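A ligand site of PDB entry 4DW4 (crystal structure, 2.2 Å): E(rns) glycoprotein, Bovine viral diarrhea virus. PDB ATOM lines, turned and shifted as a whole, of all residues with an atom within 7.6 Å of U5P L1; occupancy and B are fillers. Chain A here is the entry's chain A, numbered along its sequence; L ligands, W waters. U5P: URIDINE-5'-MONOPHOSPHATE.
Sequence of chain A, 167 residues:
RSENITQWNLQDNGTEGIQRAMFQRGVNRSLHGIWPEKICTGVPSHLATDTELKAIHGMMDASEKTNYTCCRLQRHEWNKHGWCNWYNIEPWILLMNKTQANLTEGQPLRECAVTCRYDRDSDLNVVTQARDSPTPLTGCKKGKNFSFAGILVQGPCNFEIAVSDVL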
ATOM      1  N   ILE A   5     -29.914  32.756  -1.739  1.00  0.00           N
ATOM      2  CA  ILE A   5     -28.475  32.698  -1.776  1.00  0.00           C
ATOM      3  C   ILE A   5     -28.067  33.478  -3.024  1.00  0.00           C
ATOM      4  O   ILE A   5     -28.539  33.154  -4.098  1.00  0.00           O
ATOM      5  CB  ILE A   5     -27.975  31.240  -1.863  1.00  0.00           C
ATOM      6  CG1 ILE A   5     -28.314  30.434  -0.588  1.00  0.00           C
ATOM      7  CG2 ILE A   5     -26.439  31.201  -2.177  1.00  0.00           C
ATOM      8  CD1 ILE A   5     -28.108  28.934  -0.760  1.00  0.00           C
ATOM      9  N   GLN A   7     -24.808  34.278  -5.310  1.00  0.00           N
ATOM     10  CA  GLN A   7     -23.449  33.762  -5.532  1.00  0.00           C
ATOM     11  C   GLN A   7     -22.881  34.395  -6.794  1.00  0.00           C
ATOM     12  O   GLN A   7     -23.622  34.629  -7.756  1.00  0.00           O
ATOM     13  CB  GLN A   7     -23.463  32.240  -5.687  1.00  0.00           C
ATOM     14  CG  GLN A   7     -22.051  31.573  -5.841  1.00  0.00           C
ATOM     15  CD  GLN A   7     -22.044  30.147  -5.375  1.00  0.00           C
ATOM     16  OE1 GLN A   7     -22.650  29.801  -4.354  1.00  0.00           O
ATOM     17  NE2 GLN A   7     -21.426  29.258  -6.163  1.00  0.00           N
ATOM     18  N   HIS A  32     -23.553  34.906 -10.603  1.00  0.00           N
ATOM     19  CA  HIS A  32     -23.841  33.522 -11.020  1.00  0.00           C
ATOM     20  C   HIS A  32     -25.341  33.264 -10.917  1.00  0.00           C
ATOM     21  O   HIS A  32     -25.965  32.868 -11.903  1.00  0.00           O
ATOM     22  CB  HIS A  32     -23.022  32.505 -10.205  1.00  0.00           C
ATOM     23  CG  HIS A  32     -23.128  31.089 -10.685  1.00  0.00           C
ATOM     24  ND1 HIS A  32     -22.214  30.133 -10.279  1.00  0.00           N
ATOM     25  CD2 HIS A  32     -24.024  30.504 -11.524  1.00  0.00           C
ATOM     26  CE1 HIS A  32     -22.572  29.011 -10.872  1.00  0.00           C
ATOM     27  NE2 HIS A  32     -23.670  29.178 -11.605  1.00  0.00           N
ATOM     28  N   GLY A  33     -25.911  33.500  -9.736  1.00  0.00           N
ATOM     29  CA  GLY A  33     -27.339  33.370  -9.513  1.00  0.00           C
ATOM     30  C   GLY A  33     -27.844  33.889  -8.194  1.00  0.00           C
ATOM     31  O   GLY A  33     -27.070  34.224  -7.285  1.00  0.00           O
ATOM     32  N   ILE A  34     -29.168  33.978  -8.092  1.00  0.00           N
ATOM     33  CA  ILE A  34     -29.914  34.344  -6.887  1.00  0.00           C
ATOM     34  C   ILE A  34     -30.853  33.158  -6.696  1.00  0.00           C
ATOM     35  O   ILE A  34     -31.766  32.931  -7.490  1.00  0.00           O
ATOM     36  CB  ILE A  34     -30.646  35.691  -6.968  1.00  0.00           C
ATOM     37  CG1 ILE A  34     -29.649  36.847  -7.287  1.00  0.00           C
ATOM     38  CG2 ILE A  34     -31.429  35.942  -5.653  1.00  0.00           C
ATOM     39  CD1 ILE A  34     -30.308  38.115  -7.647  1.00  0.00           C
ATOM     40  N   TRP A  35     -30.575  32.369  -5.653  1.00  0.00           N
ATOM     41  CA  TRP A  35     -31.272  31.110  -5.460  1.00  0.00           C
ATOM     42  C   TRP A  35     -32.217  30.952  -4.278  1.00  0.00           C
ATOM     43  O   TRP A  35     -31.746  30.601  -3.189  1.00  0.00           O
ATOM     44  CB  TRP A  35     -30.275  29.946  -5.481  1.00  0.00           C
ATOM     45  CG  TRP A  35     -29.300  29.933  -6.625  1.00  0.00           C
ATOM     46  CD1 TRP A  35     -29.589  30.130  -7.947  1.00  0.00           C
ATOM     47  CD2 TRP A  35     -27.896  29.640  -6.543  1.00  0.00           C
ATOM     48  NE1 TRP A  35     -28.427  30.037  -8.683  1.00  0.00           N
ATOM     49  CE2 TRP A  35     -27.393  29.686  -7.859  1.00  0.00           C
ATOM     50  CE3 TRP A  35     -26.988  29.472  -5.470  1.00  0.00           C
ATOM     51  CZ2 TRP A  35     -26.033  29.463  -8.135  1.00  0.00           C
ATOM     52  CZ3 TRP A  35     -25.676  29.174  -5.746  1.00  0.00           C
ATOM     53  CH2 TRP A  35     -25.186  29.216  -7.067  1.00  0.00           C
ATOM     54  N   PRO A  36     -33.551  31.025  -4.533  1.00  0.00           N
ATOM     55  CA  PRO A  36     -34.529  30.653  -3.506  1.00  0.00           C
ATOM     56  C   PRO A  36     -34.460  29.133  -3.294  1.00  0.00           C
ATOM     57  O   PRO A  36     -33.780  28.444  -4.059  1.00  0.00           O
ATOM     58  CB  PRO A  36     -35.865  30.993  -4.165  1.00  0.00           C
ATOM     59  CG  PRO A  36     -35.512  31.968  -5.219  1.00  0.00           C
ATOM     60  CD  PRO A  36     -34.255  31.434  -5.761  1.00  0.00           C
ATOM     61  N   GLU A  37     -35.154  28.604  -2.287  1.00  0.00           N
ATOM     62  CA  GLU A  37     -35.140  27.153  -2.029  1.00  0.00           C
ATOM     63  C   GLU A  37     -35.788  26.343  -3.133  1.00  0.00           C
ATOM     64  O   GLU A  37     -35.266  25.308  -3.526  1.00  0.00           O
ATOM     65  CB  GLU A  37     -35.708  26.807  -0.648  1.00  0.00           C
ATOM     66  CG  GLU A  37     -34.614  26.315   0.279  1.00  0.00           C
ATOM     67  CD  GLU A  37     -35.080  25.927   1.654  1.00  0.00           C
ATOM     68  OE1 GLU A  37     -34.896  26.727   2.598  1.00  0.00           O
ATOM     69  OE2 GLU A  37     -35.631  24.805   1.783  1.00  0.00           O
ATOM     70  N   ILE A  39     -36.609  24.992  -6.731  1.00  0.00           N
ATOM     71  CA  ILE A  39     -36.000  24.822  -8.046  1.00  0.00           C
ATOM     72  C   ILE A  39     -37.153  24.601  -9.046  1.00  0.00           C
ATOM     73  O   ILE A  39     -38.084  23.830  -8.777  1.00  0.00           O
ATOM     74  CB  ILE A  39     -34.887  23.728  -8.099  1.00  0.00           C
ATOM     75  CG1 ILE A  39     -33.573  24.266  -7.454  1.00  0.00           C
ATOM     76  CG2 ILE A  39     -34.639  23.218  -9.534  1.00  0.00           C
ATOM     77  CD1 ILE A  39     -32.379  23.249  -7.348  1.00  0.00           C
ATOM     78  N   LEU A  73     -25.810  31.148 -19.454  1.00  0.00           N
ATOM     79  CA  LEU A  73     -25.939  31.079 -18.004  1.00  0.00           C
ATOM     80  C   LEU A  73     -27.167  31.859 -17.574  1.00  0.00           C
ATOM     81  O   LEU A  73     -27.943  31.352 -16.763  1.00  0.00           O
ATOM     82  CB  LEU A  73     -24.667  31.596 -17.293  1.00  0.00           C
ATOM     83  CG  LEU A  73     -24.657  31.578 -15.732  1.00  0.00           C
ATOM     84  CD1 LEU A  73     -24.787  30.150 -15.172  1.00  0.00           C
ATOM     85  CD2 LEU A  73     -23.442  32.319 -15.161  1.00  0.00           C
ATOM     86  N   HIS A  76     -30.227  29.776 -18.325  1.00  0.00           N
ATOM     87  CA  HIS A  76     -30.184  28.642 -17.401  1.00  0.00           C
ATOM     88  C   HIS A  76     -30.709  29.056 -16.027  1.00  0.00           C
ATOM     89  O   HIS A  76     -31.600  28.421 -15.496  1.00  0.00           O
ATOM     90  CB  HIS A  76     -28.751  28.074 -17.336  1.00  0.00           C
ATOM     91  CG  HIS A  76     -28.569  27.060 -16.251  1.00  0.00           C
ATOM     92  ND1 HIS A  76     -29.137  25.791 -16.352  1.00  0.00           N
ATOM     93  CD2 HIS A  76     -27.982  27.199 -15.036  1.00  0.00           C
ATOM     94  CE1 HIS A  76     -28.825  25.185 -15.215  1.00  0.00           C
ATOM     95  NE2 HIS A  76     -28.137  25.973 -14.389  1.00  0.00           N
ATOM     96  N   GLU A  77     -30.260  30.225 -15.525  1.00  0.00           N
ATOM     97  CA  GLU A  77     -30.715  30.782 -14.246  1.00  0.00           C
ATOM     98  C   GLU A  77     -32.193  31.094 -14.210  1.00  0.00           C
ATOM     99  O   GLU A  77     -32.871  30.767 -13.223  1.00  0.00           O
ATOM    100  CB  GLU A  77     -29.867  31.999 -13.842  1.00  0.00           C
ATOM    101  CG  GLU A  77     -28.429  31.628 -13.536  1.00  0.00           C
ATOM    102  CD  GLU A  77     -28.250  30.552 -12.474  1.00  0.00           C
ATOM    103  OE1 GLU A  77     -28.947  30.607 -11.437  1.00  0.00           O
ATOM    104  OE2 GLU A  77     -27.399  29.651 -12.681  1.00  0.00           O
ATOM    105  N   LYS A  80     -34.104  27.450 -14.391  1.00  0.00           N
ATOM    106  CA  LYS A  80     -33.946  26.601 -13.209  1.00  0.00           C
ATOM    107  C   LYS A  80     -34.334  27.316 -11.926  1.00  0.00           C
ATOM    108  O   LYS A  80     -34.790  26.638 -10.988  1.00  0.00           O
ATOM    109  CB  LYS A  80     -32.481  26.121 -13.135  1.00  0.00           C
ATOM    110  CG  LYS A  80     -32.284  24.955 -12.176  1.00  0.00           C
ATOM    111  CD  LYS A  80     -30.852  24.551 -12.074  1.00  0.00           C
ATOM    112  CE  LYS A  80     -30.633  23.572 -10.970  1.00  0.00           C
ATOM    113  NZ  LYS A  80     -29.228  23.082 -11.000  1.00  0.00           N
ATOM    114  N   HIS A  81     -34.101  28.636 -11.832  1.00  0.00           N
ATOM    115  CA  HIS A  81     -34.376  29.337 -10.545  1.00  0.00           C
ATOM    116  C   HIS A  81     -35.285  30.536 -10.599  1.00  0.00           C
ATOM    117  O   HIS A  81     -35.619  31.061  -9.532  1.00  0.00           O
ATOM    118  CB  HIS A  81     -33.053  29.776  -9.887  1.00  0.00           C
ATOM    119  CG  HIS A  81     -32.057  28.674  -9.683  1.00  0.00           C
ATOM    120  ND1 HIS A  81     -32.152  27.788  -8.614  1.00  0.00           N
ATOM    121  CD2 HIS A  81     -30.989  28.323 -10.439  1.00  0.00           C
ATOM    122  CE1 HIS A  81     -31.138  26.956  -8.745  1.00  0.00           C
ATOM    123  NE2 HIS A  81     -30.407  27.229  -9.830  1.00  0.00           N
ATOM    124  N   VAL A 114     -16.685  30.215  -1.543  1.00  0.00           N
ATOM    125  CA  VAL A 114     -17.397  28.998  -1.890  1.00  0.00           C
ATOM    126  C   VAL A 114     -16.384  28.024  -2.448  1.00  0.00           C
ATOM    127  O   VAL A 114     -16.251  26.907  -1.943  1.00  0.00           O
ATOM    128  CB  VAL A 114     -18.575  29.246  -2.876  1.00  0.00           C
ATOM    129  CG1 VAL A 114     -19.283  27.940  -3.202  1.00  0.00           C
ATOM    130  CG2 VAL A 114     -19.570  30.232  -2.293  1.00  0.00           C
ATOM    131  N   THR A 115     -15.711  28.430  -3.528  1.00  0.00           N
ATOM    132  CA  THR A 115     -14.690  27.640  -4.196  1.00  0.00           C
ATOM    133  C   THR A 115     -13.432  28.460  -4.307  1.00  0.00           C
ATOM    134  O   THR A 115     -13.516  29.687  -4.506  1.00  0.00           O
ATOM    135  CB  THR A 115     -15.146  27.142  -5.567  1.00  0.00           C
ATOM    136  OG1 THR A 115     -15.302  28.250  -6.463  1.00  0.00           O
ATOM    137  CG2 THR A 115     -16.460  26.334  -5.506  1.00  0.00           C
ATOM    138  N   GLN A 129     -15.338  31.570  -6.633  1.00  0.00           N
ATOM    139  CA  GLN A 129     -16.785  31.818  -6.438  1.00  0.00           C
ATOM    140  C   GLN A 129     -17.043  32.175  -4.995  1.00  0.00           C
ATOM    141  O   GLN A 129     -16.416  31.586  -4.106  1.00  0.00           O
ATOM    142  CB  GLN A 129     -17.699  30.665  -6.866  1.00  0.00           C
ATOM    143  CG  GLN A 129     -17.835  30.515  -8.369  1.00  0.00           C
ATOM    144  CD  GLN A 129     -19.078  29.748  -8.761  1.00  0.00           C
ATOM    145  OE1 GLN A 129     -20.227  30.186  -8.596  1.00  0.00           O
ATOM    146  NE2 GLN A 129     -18.857  28.566  -9.258  1.00  0.00           N
ATOM    147  N   ARG A 131     -20.312  33.959  -2.108  1.00  0.00           N
ATOM    148  CA  ARG A 131     -21.740  34.204  -1.838  1.00  0.00           C
ATOM    149  C   ARG A 131     -21.882  35.093  -0.617  1.00  0.00           C
ATOM    150  O   ARG A 131     -20.895  35.432   0.033  1.00  0.00           O
ATOM    151  CB  ARG A 131     -22.537  32.890  -1.688  1.00  0.00           C
ATOM    152  CG  ARG A 131     -22.018  31.981  -0.603  1.00  0.00           C
ATOM    153  CD  ARG A 131     -22.996  30.884  -0.298  1.00  0.00           C
ATOM    154  NE  ARG A 131     -23.133  29.988  -1.436  1.00  0.00           N
ATOM    155  CZ  ARG A 131     -23.808  28.845  -1.379  1.00  0.00           C
ATOM    156  NH1 ARG A 131     -24.350  28.450  -0.235  1.00  0.00           N
ATOM    157  NH2 ARG A 131     -23.921  28.091  -2.468  1.00  0.00           N
ATOM    158  N   THR A 135     -20.667  28.950   3.914  1.00  0.00           N
ATOM    159  CA  THR A 135     -21.014  27.618   3.402  1.00  0.00           C
ATOM    160  C   THR A 135     -19.758  26.710   3.359  1.00  0.00           C
ATOM    161  O   THR A 135     -18.637  27.230   3.253  1.00  0.00           O
ATOM    162  CB  THR A 135     -21.648  27.752   1.984  1.00  0.00           C
ATOM    163  OG1 THR A 135     -22.363  26.552   1.650  1.00  0.00           O
ATOM    164  CG2 THR A 135     -20.605  28.062   0.895  1.00  0.00           C
HETATM  165  N1  U5P L   1     -25.594  25.698  -5.930  1.00  0.00           N
HETATM  166  C2  U5P L   1     -25.584  25.812  -4.561  1.00  0.00           C
HETATM  167  N3  U5P L   1     -26.725  26.179  -3.916  1.00  0.00           N
HETATM  168  C4  U5P L   1     -27.921  26.392  -4.551  1.00  0.00           C
HETATM  169  C5  U5P L   1     -27.970  26.253  -5.983  1.00  0.00           C
HETATM  170  C6  U5P L   1     -26.809  25.904  -6.611  1.00  0.00           C
HETATM  171  O2  U5P L   1     -24.573  25.610  -3.904  1.00  0.00           O
HETATM  172  O4  U5P L   1     -28.962  26.700  -3.874  1.00  0.00           O
HETATM  173  C1' U5P L   1     -24.367  25.310  -6.681  1.00  0.00           C
HETATM  174  C2' U5P L   1     -24.650  23.937  -7.330  1.00  0.00           C
HETATM  175  O2' U5P L   1     -24.111  22.949  -6.443  1.00  0.00           O
HETATM  176  C3' U5P L   1     -23.874  23.992  -8.627  1.00  0.00           C
HETATM  177  C4' U5P L   1     -23.792  25.499  -8.956  1.00  0.00           C
HETATM  178  O3' U5P L   1     -22.569  23.475  -8.452  1.00  0.00           O
HETATM  179  O4' U5P L   1     -24.050  26.220  -7.753  1.00  0.00           O
HETATM  180  C5' U5P L   1     -24.847  25.798 -10.038  1.00  0.00           C
HETATM  181  O5' U5P L   1     -26.099  26.099  -9.484  1.00  0.00           O
HETATM  182  P   U5P L   1     -27.045  26.430 -10.717  1.00  0.00           P
HETATM  183  O1P U5P L   1     -28.230  25.769 -10.322  1.00  0.00           O
HETATM  184  O2P U5P L   1     -26.728  25.875 -12.152  1.00  0.00           O
HETATM  185  O3P U5P L   1     -27.203  28.043 -10.807  1.00  0.00           O
HETATM  186  N1  U5P L   2     -18.410  27.260 -13.484  1.00  0.00           N
HETATM  187  C2  U5P L   2     -18.157  28.444 -12.807  1.00  0.00           C
HETATM  188  N3  U5P L   2     -19.041  29.472 -12.785  1.00  0.00           N
HETATM  189  C4  U5P L   2     -20.225  29.407 -13.391  1.00  0.00           C
HETATM  190  C5  U5P L   2     -20.572  28.177 -14.092  1.00  0.00           C
HETATM  191  C6  U5P L   2     -19.655  27.162 -14.149  1.00  0.00           C
HETATM  192  O2  U5P L   2     -17.122  28.608 -12.221  1.00  0.00           O
HETATM  193  O4  U5P L   2     -21.001  30.375 -13.274  1.00  0.00           O
HETATM  194  C1' U5P L   2     -17.408  26.120 -13.537  1.00  0.00           C
HETATM  195  C2' U5P L   2     -17.522  25.076 -12.350  1.00  0.00           C
HETATM  196  O2' U5P L   2     -16.292  24.357 -12.124  1.00  0.00           O
HETATM  197  C3' U5P L   2     -18.461  24.052 -12.986  1.00  0.00           C
HETATM  198  C4' U5P L   2     -17.797  23.950 -14.381  1.00  0.00           C
HETATM  199  O3' U5P L   2     -18.463  22.826 -12.241  1.00  0.00           O
HETATM  200  O4' U5P L   2     -17.548  25.347 -14.771  1.00  0.00           O
HETATM  201  C5' U5P L   2     -18.548  23.052 -15.389  1.00  0.00           C
HETATM  202  O5' U5P L   2     -19.134  23.680 -16.548  1.00  0.00           O
HETATM  203  P   U5P L   2     -20.770  23.407 -16.551  1.00  0.00           P
HETATM  204  O1P U5P L   2     -21.504  24.574 -15.933  1.00  0.00           O
HETATM  205  O2P U5P L   2     -21.182  22.012 -15.789  1.00  0.00           O
HETATM  206  O3P U5P L   2     -21.264  23.319 -18.094  1.00  0.00           O
HETATM  207  O   HOH W   1     -25.980  22.986 -12.834  1.00  0.00           O
HETATM  208  O   HOH W   2     -21.545  26.522  -5.414  1.00  0.00           O
HETATM  209  O   HOH W   3     -21.789  21.217  -6.489  1.00  0.00           O
HETATM  210  O   HOH W   4     -31.567  25.865  -4.835  1.00  0.00           O
HETATM  211  O   HOH W   5     -24.614  27.177 -13.538  1.00  0.00           O
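The side-chain carboxylate (OE2) of Glu 77 lies close to an oxygen (O3P) of U5P L1 (2.5 Å). NE2 of His 76 lies within hydrogen-bond range of O2P of U5P L1. NE2 of His 81 is in hydrogen-bond range of O1P of U5P L1, at 2.7 Å. The guanidinium group (NH2) of Arg 131 is in hydrogen-bond range of an oxygen (O2) of U5P L1, 2.9 Å away. The side-chain amino group (NZ) of Lys 80 lies within salt-bridge range of an oxygen (O1P) of U5P L1. The indole nitrogen of Trp 35 is in hydrogen-bond range of an oxygen (O3P) of U5P L1. An oxygen (O4) of U5P L2 lies close to a ring nitrogen (ND1) of His 32 (3.2 Å). An oxygen (O2) of U5P L2 is in hydrogen-bond range of the side-chain amide nitrogen (NE2) of Gln 129 (3.4 Å).
OE1 of Glu 77 is in hydrogen-bond range of NE1 of Trp 35, 2.9 Å away. The guanidinium group of Arg 131 lies within hydrogen-bond range of the side-chain amide oxygen of Gln 7 (2.8 Å). The guanidinium group of Arg 131 is in hydrogen-bond range of the side-chain hydroxyl of Thr 135 (3.3 Å). The backbone NH (N) of Trp 35 is in hydrogen-bond range of the backbone carbonyl oxygen (O) of Ile 5 (2.7 Å). The backbone carbonyl oxygen (O) of Gln 7 is in hydrogen-bond range of the backbone NH (N) of His 32 (2.9 Å). The side-chain amide oxygen of Gln 129 is in hydrogen-bond range of a ring nitrogen (ND1) of His 32 (2.6 Å).
Merely in contact with U5P L1: His 32 (3.8 Å) and Ile 5 (3.9 Å). Of the 19 residues printed, 8 come within 4 Å of U5P L1.
Water W5 bridges an oxygen (O2P) of U5P L1 (2.8 Å) and a ring nitrogen (NE2) of His 32 (2.9 Å). Water W4 bridges O4 of U5P L1 (2.9 Å) and O of Pro 36 (3.5 Å). Water W2 lies within hydrogen-bond range of the side-chain amide nitrogen (NE2) of Gln 7 and an oxygen (O4') of U5P L1.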
